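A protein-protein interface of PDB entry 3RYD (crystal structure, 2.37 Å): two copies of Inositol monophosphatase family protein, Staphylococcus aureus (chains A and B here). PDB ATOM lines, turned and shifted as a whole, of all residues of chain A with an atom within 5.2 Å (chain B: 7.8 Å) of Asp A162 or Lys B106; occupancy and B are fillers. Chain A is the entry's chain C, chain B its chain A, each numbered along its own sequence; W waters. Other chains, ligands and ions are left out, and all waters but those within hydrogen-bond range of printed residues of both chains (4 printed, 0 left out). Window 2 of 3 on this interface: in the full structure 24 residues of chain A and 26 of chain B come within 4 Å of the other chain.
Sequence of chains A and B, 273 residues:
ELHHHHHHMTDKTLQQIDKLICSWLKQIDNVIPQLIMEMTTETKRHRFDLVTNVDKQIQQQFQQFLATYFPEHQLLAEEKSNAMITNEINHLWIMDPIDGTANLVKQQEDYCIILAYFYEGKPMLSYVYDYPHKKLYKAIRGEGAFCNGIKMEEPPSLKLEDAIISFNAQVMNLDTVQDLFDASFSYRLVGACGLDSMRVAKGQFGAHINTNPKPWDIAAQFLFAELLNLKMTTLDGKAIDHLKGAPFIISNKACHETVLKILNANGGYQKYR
The backbone carbonyl oxygen (O) of Gln B107 is in hydrogen-bond range of the side-chain amide nitrogen (NE2) of Gln A204 (2.8 Å).
NZ of Lys B106 is in hydrogen-bond range of O of Asp A162, 3.0 Å away.
The side-chain amide nitrogen (NE2) of Gln A204 lies within hydrogen-bond range of the side-chain carboxylate (OE1) of Glu B109, 2.9 Å away.
The backbone carbonyl oxygen (O) of Leu A160 is in hydrogen-bond range of the backbone NH (N) of Phe A185 (3.4 Å).
The backbone NH (N) of Phe A185 sits at hydrogen-bond distance from the backbone carbonyl oxygen (O) of Ala A163 (2.8 Å).
The side-chain amide oxygen (OE1) of Gln B107 sits close to the side-chain amide oxygen (OD1) of Asn B103, 3.1 Å away.
Ala B102 touches Phe A185 (CB to CE2, 3.8 Å).
CD2 of Phe A185 touches CE of Lys B106 (3.7 Å).
Gly A203 touches Lys B106 (O to O, 3.6 Å).
Gln A204 touches Lys B106.
Asp A162 touches just one residue of chain B: Lys B106.
Of the printed residues of chain B, Gln A204 touches Lys B106, Gln B107 and Glu B109.
Thr B101 touches none of the printed residues of chain A.
Gln B108 touches none of the printed residues of chain A.
Printed residues of chain A within 4 Å of Glu B109: Gln A204 (2.9 Å).
The nearest residue of chain B that does not touch Asp A162 is Val B105 (7.5 Å).
Hydrophobic or aromatic side chains of chain B that line the printed part of chain A: Ala B102.
Printed residues of chain A that touch a printed residue of chain B: Asp A162, Phe A185, Gly A203 and Gln A204.
Among the printed residues, 7 pairs touch across the chains.
No position is printed for both chains.
Water W4 bridges O of Gly A203 and O of Lys B106.
Water W1 lies within hydrogen-bond range of NZ of Lys B106 (2.7 Å) and O of Asp A162 (3.4 Å).
Water W3 bridges OE1 of Gln A204 (2.7 Å) and OE1 of Glu B109 (2.9 Å).
Water W2 lies within hydrogen-bond range of NZ of Lys B106 (2.7 Å) and OD1 of Asp A162 (2.7 Å).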
ATOM      1  N   LEU A 158      15.318 -13.031 -27.747  1.00  0.00           N
ATOM      2  CA  LEU A 158      14.014 -13.558 -27.318  1.00  0.00           C
ATOM      3  C   LEU A 158      13.240 -12.534 -26.505  1.00  0.00           C
ATOM      4  O   LEU A 158      13.593 -12.248 -25.356  1.00  0.00           O
ATOM      5  CB  LEU A 158      14.142 -14.854 -26.519  1.00  0.00           C
ATOM      6  CG  LEU A 158      14.529 -16.137 -27.251  1.00  0.00           C
ATOM      7  CD1 LEU A 158      14.858 -17.260 -26.265  1.00  0.00           C
ATOM      8  CD2 LEU A 158      13.401 -16.578 -28.205  1.00  0.00           C
ATOM      9  N   LYS A 159      12.183 -11.981 -27.107  1.00  0.00           N
ATOM     10  CA  LYS A 159      11.214 -11.197 -26.333  1.00  0.00           C
ATOM     11  C   LYS A 159      10.385 -12.097 -25.420  1.00  0.00           C
ATOM     12  O   LYS A 159      10.175 -13.261 -25.748  1.00  0.00           O
ATOM     13  CB  LYS A 159      10.305 -10.412 -27.261  1.00  0.00           C
ATOM     14  CG  LYS A 159      11.046  -9.637 -28.301  1.00  0.00           C
ATOM     15  CD  LYS A 159      10.111  -8.607 -28.882  1.00  0.00           C
ATOM     16  CE  LYS A 159       9.329  -9.109 -30.112  1.00  0.00           C
ATOM     17  NZ  LYS A 159       8.230  -8.138 -30.502  1.00  0.00           N
ATOM     18  N   LEU A 160       9.910 -11.558 -24.291  1.00  0.00           N
ATOM     19  CA  LEU A 160       9.232 -12.381 -23.286  1.00  0.00           C
ATOM     20  C   LEU A 160       8.010 -13.152 -23.837  1.00  0.00           C
ATOM     21  O   LEU A 160       7.836 -14.337 -23.571  1.00  0.00           O
ATOM     22  CB  LEU A 160       8.872 -11.584 -22.051  1.00  0.00           C
ATOM     23  CG  LEU A 160       8.307 -12.441 -20.898  1.00  0.00           C
ATOM     24  CD1 LEU A 160       9.082 -13.737 -20.621  1.00  0.00           C
ATOM     25  CD2 LEU A 160       8.187 -11.662 -19.617  1.00  0.00           C
ATOM     26  N   GLU A 161       7.208 -12.497 -24.647  1.00  0.00           N
ATOM     27  CA  GLU A 161       6.036 -13.128 -25.236  1.00  0.00           C
ATOM     28  C   GLU A 161       6.386 -14.259 -26.218  1.00  0.00           C
ATOM     29  O   GLU A 161       5.509 -15.054 -26.593  1.00  0.00           O
ATOM     30  CB  GLU A 161       5.188 -12.076 -25.933  1.00  0.00           C
ATOM     31  CG  GLU A 161       5.810 -11.561 -27.231  1.00  0.00           C
ATOM     32  CD  GLU A 161       4.968 -10.500 -27.878  1.00  0.00           C
ATOM     33  OE1 GLU A 161       4.319  -9.773 -27.100  1.00  0.00           O
ATOM     34  OE2 GLU A 161       4.921 -10.407 -29.141  1.00  0.00           O
ATOM     35  N   ASP A 162       7.645 -14.321 -26.648  1.00  0.00           N
ATOM     36  CA  ASP A 162       8.090 -15.371 -27.588  1.00  0.00           C
ATOM     37  C   ASP A 162       8.881 -16.492 -26.917  1.00  0.00           C
ATOM     38  O   ASP A 162       9.345 -17.419 -27.599  1.00  0.00           O
ATOM     39  CB  ASP A 162       8.969 -14.784 -28.692  1.00  0.00           C
ATOM     40  CG  ASP A 162       8.201 -13.948 -29.659  1.00  0.00           C
ATOM     41  OD1 ASP A 162       7.117 -14.366 -30.075  1.00  0.00           O
ATOM     42  OD2 ASP A 162       8.681 -12.855 -30.034  1.00  0.00           O
ATOM     43  N   ALA A 163       9.069 -16.384 -25.609  1.00  0.00           N
ATOM     44  CA  ALA A 163       9.935 -17.315 -24.890  1.00  0.00           C
ATOM     45  C   ALA A 163       9.255 -18.129 -23.803  1.00  0.00           C
ATOM     46  O   ALA A 163       8.290 -17.712 -23.176  1.00  0.00           O
ATOM     47  CB  ALA A 163      11.117 -16.552 -24.257  1.00  0.00           C
ATOM     48  N   ILE A 164       9.845 -19.287 -23.550  1.00  0.00           N
ATOM     49  CA  ILE A 164       9.495 -20.121 -22.413  1.00  0.00           C
ATOM     50  C   ILE A 164      10.303 -19.695 -21.210  1.00  0.00           C
ATOM     51  O   ILE A 164      11.519 -19.507 -21.284  1.00  0.00           O
ATOM     52  CB  ILE A 164       9.817 -21.568 -22.705  1.00  0.00           C
ATOM     53  CG1 ILE A 164       8.895 -22.063 -23.838  1.00  0.00           C
ATOM     54  CG2 ILE A 164       9.626 -22.400 -21.457  1.00  0.00           C
ATOM     55  CD1 ILE A 164       8.980 -23.546 -24.097  1.00  0.00           C
ATOM     56  N   PHE A 185       5.625 -16.858 -23.443  1.00  0.00           N
ATOM     57  CA  PHE A 185       5.064 -17.829 -24.378  1.00  0.00           C
ATOM     58  C   PHE A 185       4.561 -19.107 -23.668  1.00  0.00           C
ATOM     59  O   PHE A 185       3.479 -19.609 -23.923  1.00  0.00           O
ATOM     60  CB  PHE A 185       6.073 -18.214 -25.453  1.00  0.00           C
ATOM     61  CG  PHE A 185       5.538 -19.206 -26.429  1.00  0.00           C
ATOM     62  CD1 PHE A 185       4.842 -18.788 -27.546  1.00  0.00           C
ATOM     63  CD2 PHE A 185       5.717 -20.581 -26.218  1.00  0.00           C
ATOM     64  CE1 PHE A 185       4.342 -19.728 -28.476  1.00  0.00           C
ATOM     65  CE2 PHE A 185       5.209 -21.520 -27.127  1.00  0.00           C
ATOM     66  CZ  PHE A 185       4.516 -21.091 -28.242  1.00  0.00           C
ATOM     67  N   GLY A 203      19.277 -20.823 -25.663  1.00  0.00           N
ATOM     68  CA  GLY A 203      18.164 -20.273 -26.434  1.00  0.00           C
ATOM     69  C   GLY A 203      16.817 -20.993 -26.287  1.00  0.00           C
ATOM     70  O   GLY A 203      15.803 -20.578 -26.883  1.00  0.00           O
ATOM     71  N   GLN A 204      16.799 -22.053 -25.482  1.00  0.00           N
ATOM     72  CA  GLN A 204      15.590 -22.884 -25.237  1.00  0.00           C
ATOM     73  C   GLN A 204      14.568 -22.216 -24.297  1.00  0.00           C
ATOM     74  O   GLN A 204      13.324 -22.338 -24.482  1.00  0.00           O
ATOM     75  CB  GLN A 204      16.004 -24.245 -24.651  1.00  0.00           C
ATOM     76  CG  GLN A 204      16.819 -25.117 -25.619  1.00  0.00           C
ATOM     77  CD  GLN A 204      17.365 -26.373 -24.957  1.00  0.00           C
ATOM     78  OE1 GLN A 204      18.030 -26.302 -23.924  1.00  0.00           O
ATOM     79  NE2 GLN A 204      17.083 -27.530 -25.554  1.00  0.00           N
ATOM     80  N   MET B  39      12.960 -25.810 -40.353  1.00  0.00           N
ATOM     81  CA  MET B  39      11.790 -25.563 -39.541  1.00  0.00           C
ATOM     82  C   MET B  39      11.680 -24.085 -39.185  1.00  0.00           C
ATOM     83  O   MET B  39      12.693 -23.425 -38.920  1.00  0.00           O
ATOM     84  CB  MET B  39      11.897 -26.359 -38.234  1.00  0.00           C
ATOM     85  CG  MET B  39      10.856 -26.013 -37.211  1.00  0.00           C
ATOM     86  SD  MET B  39      10.931 -26.905 -35.651  1.00  0.00           S
ATOM     87  CE  MET B  39      12.172 -25.922 -34.800  1.00  0.00           C
ATOM     88  N   LEU B  50      -0.248 -25.484 -32.418  1.00  0.00           N
ATOM     89  CA  LEU B  50       0.903 -25.229 -33.260  1.00  0.00           C
ATOM     90  C   LEU B  50       1.152 -26.420 -34.185  1.00  0.00           C
ATOM     91  O   LEU B  50       0.861 -27.564 -33.838  1.00  0.00           O
ATOM     92  CB  LEU B  50       2.105 -25.059 -32.335  1.00  0.00           C
ATOM     93  CG  LEU B  50       3.194 -24.006 -32.511  1.00  0.00           C
ATOM     94  CD1 LEU B  50       2.657 -22.597 -32.939  1.00  0.00           C
ATOM     95  CD2 LEU B  50       3.965 -23.954 -31.203  1.00  0.00           C
ATOM     96  N   GLY B 100       4.381 -32.354 -28.091  1.00  0.00           N
ATOM     97  CA  GLY B 100       5.261 -31.316 -27.575  1.00  0.00           C
ATOM     98  C   GLY B 100       5.769 -30.408 -28.681  1.00  0.00           C
ATOM     99  O   GLY B 100       6.939 -30.065 -28.728  1.00  0.00           O
ATOM    100  N   THR B 101       4.892 -30.031 -29.587  1.00  0.00           N
ATOM    101  CA  THR B 101       5.240 -29.108 -30.651  1.00  0.00           C
ATOM    102  C   THR B 101       5.820 -27.758 -30.185  1.00  0.00           C
ATOM    103  O   THR B 101       6.718 -27.242 -30.828  1.00  0.00           O
ATOM    104  CB  THR B 101       4.008 -28.784 -31.478  1.00  0.00           C
ATOM    105  OG1 THR B 101       3.345 -30.006 -31.840  1.00  0.00           O
ATOM    106  CG2 THR B 101       4.406 -28.027 -32.724  1.00  0.00           C
ATOM    107  N   ALA B 102       5.291 -27.153 -29.130  1.00  0.00           N
ATOM    108  CA  ALA B 102       5.930 -25.941 -28.589  1.00  0.00           C
ATOM    109  C   ALA B 102       7.385 -26.225 -28.208  1.00  0.00           C
ATOM    110  O   ALA B 102       8.257 -25.414 -28.489  1.00  0.00           O
ATOM    111  CB  ALA B 102       5.149 -25.325 -27.383  1.00  0.00           C
ATOM    112  N   ASN B 103       7.627 -27.378 -27.581  1.00  0.00           N
ATOM    113  CA  ASN B 103       8.996 -27.773 -27.209  1.00  0.00           C
ATOM    114  C   ASN B 103       9.931 -27.884 -28.366  1.00  0.00           C
ATOM    115  O   ASN B 103      11.052 -27.392 -28.296  1.00  0.00           O
ATOM    116  CB  ASN B 103       9.014 -29.064 -26.361  1.00  0.00           C
ATOM    117  CG  ASN B 103       8.533 -28.814 -24.935  1.00  0.00           C
ATOM    118  OD1 ASN B 103       8.484 -27.646 -24.473  1.00  0.00           O
ATOM    119  ND2 ASN B 103       8.202 -29.888 -24.223  1.00  0.00           N
ATOM    120  N   LEU B 104       9.473 -28.544 -29.421  1.00  0.00           N
ATOM    121  CA  LEU B 104      10.212 -28.681 -30.668  1.00  0.00           C
ATOM    122  C   LEU B 104      10.578 -27.306 -31.169  1.00  0.00           C
ATOM    123  O   LEU B 104      11.719 -27.050 -31.523  1.00  0.00           O
ATOM    124  CB  LEU B 104       9.349 -29.401 -31.737  1.00  0.00           C
ATOM    125  CG  LEU B 104       9.776 -29.398 -33.221  1.00  0.00           C
ATOM    126  CD1 LEU B 104      11.151 -30.020 -33.449  1.00  0.00           C
ATOM    127  CD2 LEU B 104       8.739 -30.114 -34.127  1.00  0.00           C
ATOM    128  N   VAL B 105       9.596 -26.404 -31.176  1.00  0.00           N
ATOM    129  CA  VAL B 105       9.780 -25.120 -31.875  1.00  0.00           C
ATOM    130  C   VAL B 105      10.715 -24.170 -31.142  1.00  0.00           C
ATOM    131  O   VAL B 105      11.569 -23.538 -31.765  1.00  0.00           O
ATOM    132  CB  VAL B 105       8.437 -24.482 -32.204  1.00  0.00           C
ATOM    133  CG1 VAL B 105       8.580 -22.995 -32.516  1.00  0.00           C
ATOM    134  CG2 VAL B 105       7.812 -25.242 -33.392  1.00  0.00           C
ATOM    135  N   LYS B 106      10.586 -24.144 -29.822  1.00  0.00           N
ATOM    136  CA  LYS B 106      11.311 -23.221 -28.979  1.00  0.00           C
ATOM    137  C   LYS B 106      12.603 -23.772 -28.448  1.00  0.00           C
ATOM    138  O   LYS B 106      13.522 -23.010 -28.191  1.00  0.00           O
ATOM    139  CB  LYS B 106      10.410 -22.830 -27.801  1.00  0.00           C
ATOM    140  CG  LYS B 106       9.100 -22.139 -28.259  1.00  0.00           C
ATOM    141  CD  LYS B 106       9.343 -20.793 -28.862  1.00  0.00           C
ATOM    142  CE  LYS B 106       8.046 -20.041 -29.088  1.00  0.00           C
ATOM    143  NZ  LYS B 106       8.261 -18.801 -29.975  1.00  0.00           N
ATOM    144  N   GLN B 107      12.664 -25.092 -28.257  1.00  0.00           N
ATOM    145  CA  GLN B 107      13.756 -25.766 -27.556  1.00  0.00           C
ATOM    146  C   GLN B 107      14.505 -26.860 -28.323  1.00  0.00           C
ATOM    147  O   GLN B 107      15.644 -27.181 -27.972  1.00  0.00           O
ATOM    148  CB  GLN B 107      13.189 -26.439 -26.327  1.00  0.00           C
ATOM    149  CG  GLN B 107      12.440 -25.558 -25.372  1.00  0.00           C
ATOM    150  CD  GLN B 107      12.359 -26.215 -23.978  1.00  0.00           C
ATOM    151  OE1 GLN B 107      11.318 -26.759 -23.614  1.00  0.00           O
ATOM    152  NE2 GLN B 107      13.472 -26.204 -23.223  1.00  0.00           N
ATOM    153  N   GLN B 108      13.845 -27.492 -29.307  1.00  0.00           N
ATOM    154  CA  GLN B 108      14.371 -28.688 -30.014  1.00  0.00           C
ATOM    155  C   GLN B 108      14.789 -29.807 -29.082  1.00  0.00           C
ATOM    156  O   GLN B 108      15.815 -30.466 -29.266  1.00  0.00           O
ATOM    157  CB  GLN B 108      15.494 -28.334 -30.994  1.00  0.00           C
ATOM    158  CG  GLN B 108      15.032 -27.387 -32.065  1.00  0.00           C
ATOM    159  CD  GLN B 108      16.031 -26.317 -32.325  1.00  0.00           C
ATOM    160  OE1 GLN B 108      16.141 -25.365 -31.527  1.00  0.00           O
ATOM    161  NE2 GLN B 108      16.800 -26.451 -33.437  1.00  0.00           N
ATOM    162  N   GLU B 109      13.945 -30.036 -28.098  1.00  0.00           N
ATOM    163  CA  GLU B 109      14.168 -31.020 -27.093  1.00  0.00           C
ATOM    164  C   GLU B 109      12.819 -31.112 -26.393  1.00  0.00           C
ATOM    165  O   GLU B 109      12.057 -30.164 -26.454  1.00  0.00           O
ATOM    166  CB  GLU B 109      15.214 -30.521 -26.103  1.00  0.00           C
ATOM    167  CG  GLU B 109      15.553 -31.553 -25.043  1.00  0.00           C
ATOM    168  CD  GLU B 109      16.770 -31.198 -24.201  1.00  0.00           C
ATOM    169  OE1 GLU B 109      17.355 -30.110 -24.366  1.00  0.00           O
ATOM    170  OE2 GLU B 109      17.110 -32.019 -23.325  1.00  0.00           O
HETATM  171  O   HOH W   1      10.583 -17.742 -30.707  1.00  0.00           O
HETATM  172  O   HOH W   2       6.433 -16.942 -30.635  1.00  0.00           O
HETATM  173  O   HOH W   3      18.993 -28.431 -22.657  1.00  0.00           O
HETATM  174  O   HOH W   4      13.373 -20.370 -27.852  1.00  0.00           O
